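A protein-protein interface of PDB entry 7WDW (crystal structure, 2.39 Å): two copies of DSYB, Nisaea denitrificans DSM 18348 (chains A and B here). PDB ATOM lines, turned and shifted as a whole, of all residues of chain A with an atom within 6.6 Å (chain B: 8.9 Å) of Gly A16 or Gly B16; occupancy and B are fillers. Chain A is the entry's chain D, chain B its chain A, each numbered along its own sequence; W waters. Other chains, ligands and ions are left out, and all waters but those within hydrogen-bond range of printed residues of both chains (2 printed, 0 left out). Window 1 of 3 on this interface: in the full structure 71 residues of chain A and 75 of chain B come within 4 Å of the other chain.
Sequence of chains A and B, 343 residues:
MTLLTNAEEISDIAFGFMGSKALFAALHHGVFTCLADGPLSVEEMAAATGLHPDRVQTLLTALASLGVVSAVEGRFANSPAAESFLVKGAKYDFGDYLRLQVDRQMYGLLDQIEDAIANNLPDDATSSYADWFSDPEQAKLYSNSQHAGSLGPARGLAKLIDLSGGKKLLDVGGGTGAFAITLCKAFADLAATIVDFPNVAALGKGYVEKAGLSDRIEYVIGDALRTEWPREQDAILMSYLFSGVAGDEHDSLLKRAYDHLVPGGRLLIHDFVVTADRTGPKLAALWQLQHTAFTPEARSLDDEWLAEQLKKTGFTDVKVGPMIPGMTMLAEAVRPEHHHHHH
Water W1 lies within hydrogen-bond range of the backbone carbonyl oxygen (O) of Gly A16 (2.6 Å), the backbone carbonyl oxygen (O) of Ile B13 (3.0 Å) and the backbone NH (N) of Ser A20 (3.5 Å).
The backbone carbonyl oxygen (O) of Val B102 is in hydrogen-bond range of the backbone NH (N) of Tyr B107, at 3.0 Å.
OG of Ser B20 is in hydrogen-bond range of O of Gly B16 (3.4 Å).
Of the 24 printed residues of chain B, 20 touch a printed residue of chain A.
Hydrophobic or aromatic side chains of chain A within 4 Å of the printed part of chain B: Ile A13, Ala A14, Phe A15, Phe A17, Met A18, Leu A66, Leu A283 and Leu A286.
Gly A16 touches just these residues of chain B: Gly B16 (3.8 Å) and Ser B20 (3.2 Å).
Of the printed residues of chain B, Leu A283 touches Ser B11 (3.6 Å) and Asp B12 (3.7 Å).
Of the printed residues of chain A, Ala B14 touches Ser A20.
Gly B16 touches just these residues of chain A: Gly A16 (3.8 Å), Phe A17 (3.8 Å) and Ser A20 (3.2 Å).
Printed residues of chain A within 4 Å of Phe B17: Phe A17 and Ser A20.
The nearest residue of chain A that does not touch Gly B16 is Ile A13 (4.6 Å).
The backbone carbonyl oxygen of Ile B13 sits at hydrogen-bond distance from the side-chain hydroxyl of Ser A20 (2.9 Å).
OG of Ser A20 is in hydrogen-bond range of O of Ala B14, at 3.2 Å.
O of Leu A286 sits close to SD of Met B18 (3.5 Å).
N of Gly A16 lies within hydrogen-bond range of OG of Ser B20 (3.2 Å).
The side-chain hydroxyl (OG) of Ser B20 is in hydrogen-bond range of the backbone NH (N) of Phe A17 (2.9 Å).
N of Gly B16 is in hydrogen-bond range of OG of Ser A20 (3.2 Å).
The side-chain hydroxyl (OG) of Ser B20 sits at hydrogen-bond distance from the backbone carbonyl oxygen (O) of Ile A13, at 2.6 Å.
The side-chain carboxylate (OD1) of Asp A12 lies within salt-bridge range of the side-chain amino group (NZ) of Lys B282 (2.8 Å).
The backbone carbonyl oxygen (O) of Ala A14 lies within hydrogen-bond range of the side-chain hydroxyl (OG) of Ser B20 (3.0 Å).
The side-chain sulfur of Met A18 lies close to the backbone carbonyl oxygen of Leu B286.
The side-chain hydroxyl of Ser A20 sits at hydrogen-bond distance from the backbone NH of Phe B17 (2.9 Å).
Phe A15 touches Ser B20, but with the chains exchanged Ser A20 does not touch Phe B15 (4.1 Å).
Gly A16 touches Ser B20, and with the chains exchanged Ser A20 touches Gly B16.
Phe B17 touches its own counterpart, Phe A17.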
ATOM      1  N   SER A  11     -15.922  -6.063  -9.757  1.00  0.00           N
ATOM      2  CA  SER A  11     -16.912  -7.115  -9.938  1.00  0.00           C
ATOM      3  C   SER A  11     -18.188  -6.834  -9.171  1.00  0.00           C
ATOM      4  O   SER A  11     -19.275  -7.069  -9.688  1.00  0.00           O
ATOM      5  CB  SER A  11     -16.354  -8.501  -9.560  1.00  0.00           C
ATOM      6  OG  SER A  11     -15.445  -8.952 -10.544  1.00  0.00           O
ATOM      7  N   ASP A  12     -18.061  -6.338  -7.945  1.00  0.00           N
ATOM      8  CA  ASP A  12     -19.243  -5.980  -7.147  1.00  0.00           C
ATOM      9  C   ASP A  12     -20.224  -5.077  -7.907  1.00  0.00           C
ATOM     10  O   ASP A  12     -21.448  -5.188  -7.751  1.00  0.00           O
ATOM     11  CB  ASP A  12     -18.832  -5.279  -5.857  1.00  0.00           C
ATOM     12  CG  ASP A  12     -18.654  -6.239  -4.704  1.00  0.00           C
ATOM     13  OD1 ASP A  12     -19.245  -7.342  -4.753  1.00  0.00           O
ATOM     14  OD2 ASP A  12     -17.921  -5.887  -3.749  1.00  0.00           O
ATOM     15  N   ILE A  13     -19.664  -4.183  -8.720  1.00  0.00           N
ATOM     16  CA  ILE A  13     -20.427  -3.173  -9.425  1.00  0.00           C
ATOM     17  C   ILE A  13     -20.915  -3.730 -10.746  1.00  0.00           C
ATOM     18  O   ILE A  13     -22.083  -3.589 -11.094  1.00  0.00           O
ATOM     19  CB  ILE A  13     -19.554  -1.941  -9.689  1.00  0.00           C
ATOM     20  CG1 ILE A  13     -19.210  -1.264  -8.366  1.00  0.00           C
ATOM     21  CG2 ILE A  13     -20.235  -0.986 -10.635  1.00  0.00           C
ATOM     22  CD1 ILE A  13     -18.484   0.049  -8.546  1.00  0.00           C
ATOM     23  N   ALA A  14     -20.002  -4.375 -11.464  1.00  0.00           N
ATOM     24  CA  ALA A  14     -20.302  -4.978 -12.752  1.00  0.00           C
ATOM     25  C   ALA A  14     -21.539  -5.868 -12.696  1.00  0.00           C
ATOM     26  O   ALA A  14     -22.399  -5.813 -13.590  1.00  0.00           O
ATOM     27  CB  ALA A  14     -19.098  -5.762 -13.257  1.00  0.00           C
ATOM     28  N   PHE A  15     -21.645  -6.660 -11.634  1.00  0.00           N
ATOM     29  CA  PHE A  15     -22.718  -7.635 -11.514  1.00  0.00           C
ATOM     30  C   PHE A  15     -23.842  -7.190 -10.582  1.00  0.00           C
ATOM     31  O   PHE A  15     -24.737  -7.976 -10.232  1.00  0.00           O
ATOM     32  CB  PHE A  15     -22.141  -8.964 -11.052  1.00  0.00           C
ATOM     33  CG  PHE A  15     -20.960  -9.425 -11.865  1.00  0.00           C
ATOM     34  CD1 PHE A  15     -20.989  -9.376 -13.250  1.00  0.00           C
ATOM     35  CD2 PHE A  15     -19.821  -9.903 -11.247  1.00  0.00           C
ATOM     36  CE1 PHE A  15     -19.894  -9.813 -14.016  1.00  0.00           C
ATOM     37  CE2 PHE A  15     -18.727 -10.337 -11.998  1.00  0.00           C
ATOM     38  CZ  PHE A  15     -18.765 -10.291 -13.390  1.00  0.00           C
ATOM     39  N   GLY A  16     -23.803  -5.922 -10.182  1.00  0.00           N
ATOM     40  CA  GLY A  16     -24.851  -5.370  -9.340  1.00  0.00           C
ATOM     41  C   GLY A  16     -26.215  -5.544  -9.973  1.00  0.00           C
ATOM     42  O   GLY A  16     -27.201  -5.760  -9.270  1.00  0.00           O
ATOM     43  N   PHE A  17     -26.255  -5.477 -11.305  1.00  0.00           N
ATOM     44  CA  PHE A  17     -27.479  -5.658 -12.076  1.00  0.00           C
ATOM     45  C   PHE A  17     -28.130  -7.033 -11.871  1.00  0.00           C
ATOM     46  O   PHE A  17     -29.347  -7.164 -11.968  1.00  0.00           O
ATOM     47  CB  PHE A  17     -27.223  -5.405 -13.571  1.00  0.00           C
ATOM     48  CG  PHE A  17     -26.625  -6.587 -14.314  1.00  0.00           C
ATOM     49  CD1 PHE A  17     -27.436  -7.615 -14.781  1.00  0.00           C
ATOM     50  CD2 PHE A  17     -25.253  -6.647 -14.579  1.00  0.00           C
ATOM     51  CE1 PHE A  17     -26.899  -8.695 -15.485  1.00  0.00           C
ATOM     52  CE2 PHE A  17     -24.704  -7.723 -15.275  1.00  0.00           C
ATOM     53  CZ  PHE A  17     -25.530  -8.751 -15.731  1.00  0.00           C
ATOM     54  N   MET A  18     -27.336  -8.056 -11.573  1.00  0.00           N
ATOM     55  CA  MET A  18     -27.925  -9.369 -11.319  1.00  0.00           C
ATOM     56  C   MET A  18     -28.739  -9.343 -10.034  1.00  0.00           C
ATOM     57  O   MET A  18     -29.760 -10.025  -9.905  1.00  0.00           O
ATOM     58  CB  MET A  18     -26.856 -10.449 -11.250  1.00  0.00           C
ATOM     59  CG  MET A  18     -26.051 -10.598 -12.523  1.00  0.00           C
ATOM     60  SD  MET A  18     -24.689 -11.758 -12.264  1.00  0.00           S
ATOM     61  CE  MET A  18     -23.844 -11.661 -13.828  1.00  0.00           C
ATOM     62  N   GLY A  19     -28.283  -8.541  -9.087  1.00  0.00           N
ATOM     63  CA  GLY A  19     -28.933  -8.462  -7.800  1.00  0.00           C
ATOM     64  C   GLY A  19     -30.224  -7.681  -7.898  1.00  0.00           C
ATOM     65  O   GLY A  19     -31.192  -8.010  -7.223  1.00  0.00           O
ATOM     66  N   SER A  20     -30.256  -6.657  -8.749  1.00  0.00           N
ATOM     67  CA  SER A  20     -31.509  -5.930  -8.951  1.00  0.00           C
ATOM     68  C   SER A  20     -32.499  -6.942  -9.467  1.00  0.00           C
ATOM     69  O   SER A  20     -33.625  -7.019  -8.990  1.00  0.00           O
ATOM     70  CB  SER A  20     -31.357  -4.793  -9.942  1.00  0.00           C
ATOM     71  OG  SER A  20     -30.241  -3.991  -9.614  1.00  0.00           O
ATOM     72  N   LYS A  21     -32.053  -7.759 -10.413  1.00  0.00           N
ATOM     73  CA  LYS A  21     -32.954  -8.727 -11.028  1.00  0.00           C
ATOM     74  C   LYS A  21     -33.415  -9.830 -10.082  1.00  0.00           C
ATOM     75  O   LYS A  21     -34.474 -10.409 -10.299  1.00  0.00           O
ATOM     76  CB  LYS A  21     -32.367  -9.303 -12.321  1.00  0.00           C
ATOM     77  CG  LYS A  21     -32.569  -8.407 -13.539  1.00  0.00           C
ATOM     78  CD  LYS A  21     -34.038  -8.433 -14.028  1.00  0.00           C
ATOM     79  CE  LYS A  21     -34.208  -7.649 -15.357  1.00  0.00           C
ATOM     80  NZ  LYS A  21     -35.557  -7.780 -16.009  1.00  0.00           N
ATOM     81  N   LEU A  66     -27.925 -11.222  -0.628  1.00  0.00           N
ATOM     82  CA  LEU A  66     -28.106  -9.784  -0.854  1.00  0.00           C
ATOM     83  C   LEU A  66     -28.620  -9.099   0.402  1.00  0.00           C
ATOM     84  O   LEU A  66     -28.534  -7.869   0.535  1.00  0.00           O
ATOM     85  CB  LEU A  66     -29.044  -9.502  -2.047  1.00  0.00           C
ATOM     86  CG  LEU A  66     -28.434  -9.799  -3.423  1.00  0.00           C
ATOM     87  CD1 LEU A  66     -29.484 -10.201  -4.438  1.00  0.00           C
ATOM     88  CD2 LEU A  66     -27.565  -8.645  -3.935  1.00  0.00           C
ATOM     89  N   LEU A 283     -27.292   7.043  -5.264  1.00  0.00           N
ATOM     90  CA  LEU A 283     -28.582   6.738  -5.874  1.00  0.00           C
ATOM     91  C   LEU A 283     -29.106   7.871  -6.760  1.00  0.00           C
ATOM     92  O   LEU A 283     -29.699   7.627  -7.820  1.00  0.00           O
ATOM     93  CB  LEU A 283     -29.620   6.322  -4.826  1.00  0.00           C
ATOM     94  CG  LEU A 283     -29.252   5.024  -4.096  1.00  0.00           C
ATOM     95  CD1 LEU A 283     -30.402   4.572  -3.223  1.00  0.00           C
ATOM     96  CD2 LEU A 283     -28.852   3.918  -5.091  1.00  0.00           C
ATOM     97  N   LEU A 286     -27.155   7.807  -9.982  1.00  0.00           N
ATOM     98  CA  LEU A 286     -27.509   6.708 -10.875  1.00  0.00           C
ATOM     99  C   LEU A 286     -28.882   6.918 -11.548  1.00  0.00           C
ATOM    100  O   LEU A 286     -29.066   6.523 -12.697  1.00  0.00           O
ATOM    101  CB  LEU A 286     -27.490   5.366 -10.130  1.00  0.00           C
ATOM    102  CG  LEU A 286     -26.162   4.844  -9.577  1.00  0.00           C
ATOM    103  CD1 LEU A 286     -26.407   3.536  -8.838  1.00  0.00           C
ATOM    104  CD2 LEU A 286     -25.079   4.678 -10.661  1.00  0.00           C
ATOM    105  N   GLU B   9     -31.760   0.828   1.800  1.00  0.00           N
ATOM    106  CA  GLU B   9     -30.911  -0.340   1.601  1.00  0.00           C
ATOM    107  C   GLU B   9     -31.507  -1.227   0.513  1.00  0.00           C
ATOM    108  O   GLU B   9     -30.796  -1.788  -0.325  1.00  0.00           O
ATOM    109  CB  GLU B   9     -30.723  -1.103   2.919  1.00  0.00           C
ATOM    110  CG  GLU B   9     -29.819  -0.383   3.916  1.00  0.00           C
ATOM    111  CD  GLU B   9     -29.639  -1.145   5.237  1.00  0.00           C
ATOM    112  OE1 GLU B   9     -30.459  -2.037   5.543  1.00  0.00           O
ATOM    113  OE2 GLU B   9     -28.677  -0.840   5.969  1.00  0.00           O
ATOM    114  N   ILE B  10     -32.826  -1.342   0.531  1.00  0.00           N
ATOM    115  CA  ILE B  10     -33.536  -1.968  -0.566  1.00  0.00           C
ATOM    116  C   ILE B  10     -33.251  -1.215  -1.854  1.00  0.00           C
ATOM    117  O   ILE B  10     -33.079  -1.820  -2.900  1.00  0.00           O
ATOM    118  CB  ILE B  10     -35.054  -2.009  -0.313  1.00  0.00           C
ATOM    119  CG1 ILE B  10     -35.386  -3.129   0.675  1.00  0.00           C
ATOM    120  CG2 ILE B  10     -35.811  -2.225  -1.606  1.00  0.00           C
ATOM    121  CD1 ILE B  10     -36.737  -2.979   1.296  1.00  0.00           C
ATOM    122  N   SER B  11     -33.198   0.108  -1.780  1.00  0.00           N
ATOM    123  CA  SER B  11     -32.950   0.898  -2.978  1.00  0.00           C
ATOM    124  C   SER B  11     -31.548   0.638  -3.531  1.00  0.00           C
ATOM    125  O   SER B  11     -31.340   0.646  -4.746  1.00  0.00           O
ATOM    126  CB  SER B  11     -33.184   2.388  -2.710  1.00  0.00           C
ATOM    127  OG  SER B  11     -34.537   2.627  -2.340  1.00  0.00           O
ATOM    128  N   ASP B  12     -30.599   0.385  -2.636  1.00  0.00           N
ATOM    129  CA  ASP B  12     -29.235   0.029  -3.027  1.00  0.00           C
ATOM    130  C   ASP B  12     -29.190  -1.195  -3.928  1.00  0.00           C
ATOM    131  O   ASP B  12     -28.446  -1.242  -4.906  1.00  0.00           O
ATOM    132  CB  ASP B  12     -28.366  -0.206  -1.791  1.00  0.00           C
ATOM    133  CG  ASP B  12     -27.960   1.089  -1.129  1.00  0.00           C
ATOM    134  OD1 ASP B  12     -27.981   2.124  -1.825  1.00  0.00           O
ATOM    135  OD2 ASP B  12     -27.617   1.078   0.073  1.00  0.00           O
ATOM    136  N   ILE B  13     -29.998  -2.185  -3.592  1.00  0.00           N
ATOM    137  CA  ILE B  13     -30.086  -3.391  -4.396  1.00  0.00           C
ATOM    138  C   ILE B  13     -30.930  -3.135  -5.660  1.00  0.00           C
ATOM    139  O   ILE B  13     -30.493  -3.407  -6.772  1.00  0.00           O
ATOM    140  CB  ILE B  13     -30.629  -4.530  -3.526  1.00  0.00           C
ATOM    141  CG1 ILE B  13     -29.619  -4.799  -2.412  1.00  0.00           C
ATOM    142  CG2 ILE B  13     -30.855  -5.771  -4.319  1.00  0.00           C
ATOM    143  CD1 ILE B  13     -30.105  -5.763  -1.388  1.00  0.00           C
ATOM    144  N   ALA B  14     -32.116  -2.575  -5.474  1.00  0.00           N
ATOM    145  CA  ALA B  14     -33.016  -2.267  -6.586  1.00  0.00           C
ATOM    146  C   ALA B  14     -32.322  -1.557  -7.754  1.00  0.00           C
ATOM    147  O   ALA B  14     -32.545  -1.892  -8.908  1.00  0.00           O
ATOM    148  CB  ALA B  14     -34.211  -1.433  -6.088  1.00  0.00           C
ATOM    149  N   PHE B  15     -31.485  -0.570  -7.463  1.00  0.00           N
ATOM    150  CA  PHE B  15     -30.901   0.227  -8.529  1.00  0.00           C
ATOM    151  C   PHE B  15     -29.440  -0.078  -8.813  1.00  0.00           C
ATOM    152  O   PHE B  15     -28.728   0.758  -9.382  1.00  0.00           O
ATOM    153  CB  PHE B  15     -31.121   1.709  -8.234  1.00  0.00           C
ATOM    154  CG  PHE B  15     -32.524   2.009  -7.837  1.00  0.00           C
ATOM    155  CD1 PHE B  15     -33.577   1.588  -8.630  1.00  0.00           C
ATOM    156  CD2 PHE B  15     -32.804   2.639  -6.648  1.00  0.00           C
ATOM    157  CE1 PHE B  15     -34.882   1.824  -8.254  1.00  0.00           C
ATOM    158  CE2 PHE B  15     -34.123   2.890  -6.270  1.00  0.00           C
ATOM    159  CZ  PHE B  15     -35.158   2.478  -7.072  1.00  0.00           C
ATOM    160  N   GLY B  16     -29.004  -1.279  -8.433  1.00  0.00           N
ATOM    161  CA  GLY B  16     -27.660  -1.743  -8.726  1.00  0.00           C
ATOM    162  C   GLY B  16     -27.394  -1.909 -10.210  1.00  0.00           C
ATOM    163  O   GLY B  16     -26.252  -1.764 -10.648  1.00  0.00           O
ATOM    164  N   PHE B  17     -28.434  -2.214 -10.993  1.00  0.00           N
ATOM    165  CA  PHE B  17     -28.273  -2.334 -12.450  1.00  0.00           C
ATOM    166  C   PHE B  17     -27.786  -1.040 -13.063  1.00  0.00           C
ATOM    167  O   PHE B  17     -27.018  -1.038 -14.030  1.00  0.00           O
ATOM    168  CB  PHE B  17     -29.544  -2.838 -13.138  1.00  0.00           C
ATOM    169  CG  PHE B  17     -30.695  -1.882 -13.088  1.00  0.00           C
ATOM    170  CD1 PHE B  17     -31.448  -1.747 -11.939  1.00  0.00           C
ATOM    171  CD2 PHE B  17     -31.036  -1.125 -14.209  1.00  0.00           C
ATOM    172  CE1 PHE B  17     -32.513  -0.864 -11.894  1.00  0.00           C
ATOM    173  CE2 PHE B  17     -32.093  -0.258 -14.175  1.00  0.00           C
ATOM    174  CZ  PHE B  17     -32.841  -0.126 -13.009  1.00  0.00           C
ATOM    175  N   MET B  18     -28.207   0.072 -12.467  1.00  0.00           N
ATOM    176  CA  MET B  18     -27.783   1.386 -12.928  1.00  0.00           C
ATOM    177  C   MET B  18     -26.272   1.589 -12.815  1.00  0.00           C
ATOM    178  O   MET B  18     -25.646   2.062 -13.750  1.00  0.00           O
ATOM    179  CB  MET B  18     -28.552   2.497 -12.206  1.00  0.00           C
ATOM    180  CG  MET B  18     -30.067   2.411 -12.360  1.00  0.00           C
ATOM    181  SD  MET B  18     -30.890   3.731 -11.481  1.00  0.00           S
ATOM    182  CE  MET B  18     -32.616   3.351 -11.778  1.00  0.00           C
ATOM    183  N   GLY B  19     -25.684   1.214 -11.680  1.00  0.00           N
ATOM    184  CA  GLY B  19     -24.233   1.282 -11.504  1.00  0.00           C
ATOM    185  C   GLY B  19     -23.470   0.379 -12.470  1.00  0.00           C
ATOM    186  O   GLY B  19     -22.469   0.796 -13.057  1.00  0.00           O
ATOM    187  N   SER B  20     -23.950  -0.855 -12.645  1.00  0.00           N
ATOM    188  CA  SER B  20     -23.365  -1.779 -13.636  1.00  0.00           C
ATOM    189  C   SER B  20     -23.305  -1.139 -15.018  1.00  0.00           C
ATOM    190  O   SER B  20     -22.319  -1.282 -15.741  1.00  0.00           O
ATOM    191  CB  SER B  20     -24.171  -3.075 -13.751  1.00  0.00           C
ATOM    192  OG  SER B  20     -24.235  -3.759 -12.526  1.00  0.00           O
ATOM    193  N   LYS B  21     -24.370  -0.433 -15.380  1.00  0.00           N
ATOM    194  CA  LYS B  21     -24.443   0.199 -16.686  1.00  0.00           C
ATOM    195  C   LYS B  21     -23.616   1.478 -16.790  1.00  0.00           C
ATOM    196  O   LYS B  21     -23.178   1.840 -17.876  1.00  0.00           O
ATOM    197  CB  LYS B  21     -25.900   0.436 -17.085  1.00  0.00           C
ATOM    198  CG  LYS B  21     -26.574  -0.780 -17.711  1.00  0.00           C
ATOM    199  CD  LYS B  21     -26.112  -0.960 -19.160  1.00  0.00           C
ATOM    200  CE  LYS B  21     -27.007  -1.926 -19.940  1.00  0.00           C
ATOM    201  NZ  LYS B  21     -26.625  -2.032 -21.386  1.00  0.00           N
ATOM    202  N   ALA B  22     -23.391   2.159 -15.675  1.00  0.00           N
ATOM    203  CA  ALA B  22     -22.417   3.256 -15.653  1.00  0.00           C
ATOM    204  C   ALA B  22     -21.015   2.752 -16.013  1.00  0.00           C
ATOM    205  O   ALA B  22     -20.316   3.327 -16.848  1.00  0.00           O
ATOM    206  CB  ALA B  22     -22.393   3.938 -14.283  1.00  0.00           C
ATOM    207  N   LEU B  23     -20.596   1.667 -15.376  1.00  0.00           N
ATOM    208  CA  LEU B  23     -19.317   1.083 -15.706  1.00  0.00           C
ATOM    209  C   LEU B  23     -19.299   0.682 -17.180  1.00  0.00           C
ATOM    210  O   LEU B  23     -18.376   1.042 -17.911  1.00  0.00           O
ATOM    211  CB  LEU B  23     -19.055  -0.138 -14.833  1.00  0.00           C
ATOM    212  CG  LEU B  23     -17.743  -0.860 -15.134  1.00  0.00           C
ATOM    213  CD1 LEU B  23     -16.573   0.010 -14.705  1.00  0.00           C
ATOM    214  CD2 LEU B  23     -17.715  -2.210 -14.438  1.00  0.00           C
ATOM    215  N   PHE B  24     -20.320  -0.063 -17.608  1.00  0.00           N
ATOM    216  CA  PHE B  24     -20.365  -0.620 -18.976  1.00  0.00           C
ATOM    217  C   PHE B  24     -20.310   0.450 -20.056  1.00  0.00           C
ATOM    218  O   PHE B  24     -19.580   0.330 -21.037  1.00  0.00           O
ATOM    219  CB  PHE B  24     -21.622  -1.476 -19.190  1.00  0.00           C
ATOM    220  CG  PHE B  24     -21.684  -2.684 -18.307  1.00  0.00           C
ATOM    221  CD1 PHE B  24     -20.535  -3.169 -17.700  1.00  0.00           C
ATOM    222  CD2 PHE B  24     -22.892  -3.320 -18.058  1.00  0.00           C
ATOM    223  CE1 PHE B  24     -20.598  -4.281 -16.870  1.00  0.00           C
ATOM    224  CE2 PHE B  24     -22.961  -4.428 -17.229  1.00  0.00           C
ATOM    225  CZ  PHE B  24     -21.813  -4.909 -16.632  1.00  0.00           C
ATOM    226  N   LEU B  66     -19.448   5.681  -7.212  1.00  0.00           N
ATOM    227  CA  LEU B  66     -19.226   4.257  -7.024  1.00  0.00           C
ATOM    228  C   LEU B  66     -17.767   3.976  -6.676  1.00  0.00           C
ATOM    229  O   LEU B  66     -17.375   2.831  -6.500  1.00  0.00           O
ATOM    230  CB  LEU B  66     -19.589   3.499  -8.291  1.00  0.00           C
ATOM    231  CG  LEU B  66     -21.034   3.626  -8.744  1.00  0.00           C
ATOM    232  CD1 LEU B  66     -21.137   3.217 -10.186  1.00  0.00           C
ATOM    233  CD2 LEU B  66     -21.894   2.753  -7.850  1.00  0.00           C
ATOM    234  N   VAL B 102     -20.527  -9.468 -20.630  1.00  0.00           N
ATOM    235  CA  VAL B 102     -21.452  -9.136 -19.546  1.00  0.00           C
ATOM    236  C   VAL B 102     -22.544  -8.133 -19.960  1.00  0.00           C
ATOM    237  O   VAL B 102     -23.718  -8.356 -19.711  1.00  0.00           O
ATOM    238  CB  VAL B 102     -20.731  -8.650 -18.271  1.00  0.00           C
ATOM    239  CG1 VAL B 102     -21.745  -8.336 -17.163  1.00  0.00           C
ATOM    240  CG2 VAL B 102     -19.771  -9.707 -17.788  1.00  0.00           C
ATOM    241  N   TYR B 107     -26.665  -8.841 -19.586  1.00  0.00           N
ATOM    242  CA  TYR B 107     -27.620  -7.840 -19.139  1.00  0.00           C
ATOM    243  C   TYR B 107     -28.988  -8.030 -19.800  1.00  0.00           C
ATOM    244  O   TYR B 107     -29.969  -8.339 -19.138  1.00  0.00           O
ATOM    245  CB  TYR B 107     -27.064  -6.442 -19.417  1.00  0.00           C
ATOM    246  CG  TYR B 107     -27.912  -5.349 -18.832  1.00  0.00           C
ATOM    247  CD1 TYR B 107     -28.986  -4.836 -19.542  1.00  0.00           C
ATOM    248  CD2 TYR B 107     -27.652  -4.832 -17.569  1.00  0.00           C
ATOM    249  CE1 TYR B 107     -29.774  -3.845 -19.023  1.00  0.00           C
ATOM    250  CE2 TYR B 107     -28.444  -3.829 -17.034  1.00  0.00           C
ATOM    251  CZ  TYR B 107     -29.509  -3.338 -17.771  1.00  0.00           C
ATOM    252  OH  TYR B 107     -30.331  -2.345 -17.278  1.00  0.00           O
ATOM    253  N   LEU B 110     -30.682 -11.403 -19.116  1.00  0.00           N
ATOM    254  CA  LEU B 110     -31.285 -11.591 -17.796  1.00  0.00           C
ATOM    255  C   LEU B 110     -32.681 -10.959 -17.733  1.00  0.00           C
ATOM    256  O   LEU B 110     -33.401 -11.140 -16.751  1.00  0.00           O
ATOM    257  CB  LEU B 110     -30.371 -11.064 -16.666  1.00  0.00           C
ATOM    258  CG  LEU B 110     -30.700 -11.475 -15.226  1.00  0.00           C
ATOM    259  CD1 LEU B 110     -30.715 -12.981 -15.089  1.00  0.00           C
ATOM    260  CD2 LEU B 110     -29.736 -10.856 -14.212  1.00  0.00           C
ATOM    261  N   LYS B 282     -22.064 -13.854  -2.337  1.00  0.00           N
ATOM    262  CA  LYS B 282     -23.010 -13.104  -3.163  1.00  0.00           C
ATOM    263  C   LYS B 282     -22.753 -13.144  -4.668  1.00  0.00           C
ATOM    264  O   LYS B 282     -23.678 -13.381  -5.427  1.00  0.00           O
ATOM    265  CB  LYS B 282     -23.104 -11.662  -2.655  1.00  0.00           C
ATOM    266  CG  LYS B 282     -23.404 -10.592  -3.682  1.00  0.00           C
ATOM    267  CD  LYS B 282     -23.305  -9.220  -2.995  1.00  0.00           C
ATOM    268  CE  LYS B 282     -22.918  -8.106  -3.951  1.00  0.00           C
ATOM    269  NZ  LYS B 282     -21.701  -7.379  -3.487  1.00  0.00           N
ATOM    270  N   LEU B 283     -21.519 -12.919  -5.103  1.00  0.00           N
ATOM    271  CA  LEU B 283     -21.213 -12.970  -6.525  1.00  0.00           C
ATOM    272  C   LEU B 283     -21.528 -14.322  -7.159  1.00  0.00           C
ATOM    273  O   LEU B 283     -22.032 -14.375  -8.280  1.00  0.00           O
ATOM    274  CB  LEU B 283     -19.760 -12.562  -6.809  1.00  0.00           C
ATOM    275  CG  LEU B 283     -19.390 -11.107  -6.506  1.00  0.00           C
ATOM    276  CD1 LEU B 283     -18.129 -10.706  -7.223  1.00  0.00           C
ATOM    277  CD2 LEU B 283     -20.544 -10.170  -6.914  1.00  0.00           C
ATOM    278  N   LEU B 286     -25.384 -14.830  -7.398  1.00  0.00           N
ATOM    279  CA  LEU B 286     -25.889 -13.963  -8.458  1.00  0.00           C
ATOM    280  C   LEU B 286     -25.618 -14.566  -9.839  1.00  0.00           C
ATOM    281  O   LEU B 286     -26.473 -14.515 -10.726  1.00  0.00           O
ATOM    282  CB  LEU B 286     -25.291 -12.551  -8.335  1.00  0.00           C
ATOM    283  CG  LEU B 286     -25.708 -11.801  -7.057  1.00  0.00           C
ATOM    284  CD1 LEU B 286     -25.413 -10.283  -7.109  1.00  0.00           C
ATOM    285  CD2 LEU B 286     -27.182 -12.049  -6.733  1.00  0.00           C
ATOM    286  N   TRP B 287     -24.435 -15.156 -10.009  1.00  0.00           N
ATOM    287  CA  TRP B 287     -24.074 -15.767 -11.276  1.00  0.00           C
ATOM    288  C   TRP B 287     -24.827 -17.081 -11.526  1.00  0.00           C
ATOM    289  O   TRP B 287     -25.064 -17.445 -12.681  1.00  0.00           O
ATOM    290  CB  TRP B 287     -22.566 -15.972 -11.368  1.00  0.00           C
ATOM    291  CG  TRP B 287     -21.860 -14.894 -12.134  1.00  0.00           C
ATOM    292  CD1 TRP B 287     -21.121 -13.864 -11.619  1.00  0.00           C
ATOM    293  CD2 TRP B 287     -21.826 -14.736 -13.558  1.00  0.00           C
ATOM    294  NE1 TRP B 287     -20.629 -13.075 -12.638  1.00  0.00           N
ATOM    295  CE2 TRP B 287     -21.046 -13.592 -13.835  1.00  0.00           C
ATOM    296  CE3 TRP B 287     -22.383 -15.451 -14.628  1.00  0.00           C
ATOM    297  CZ2 TRP B 287     -20.806 -13.150 -15.132  1.00  0.00           C
ATOM    298  CZ3 TRP B 287     -22.145 -15.011 -15.917  1.00  0.00           C
ATOM    299  CH2 TRP B 287     -21.370 -13.864 -16.159  1.00  0.00           C
HETATM  300  O   HOH W   1     -27.929  -4.875  -6.893  1.00  0.00           O
HETATM  301  O   HOH W   2     -24.020  -1.848  -9.195  1.00  0.00           O
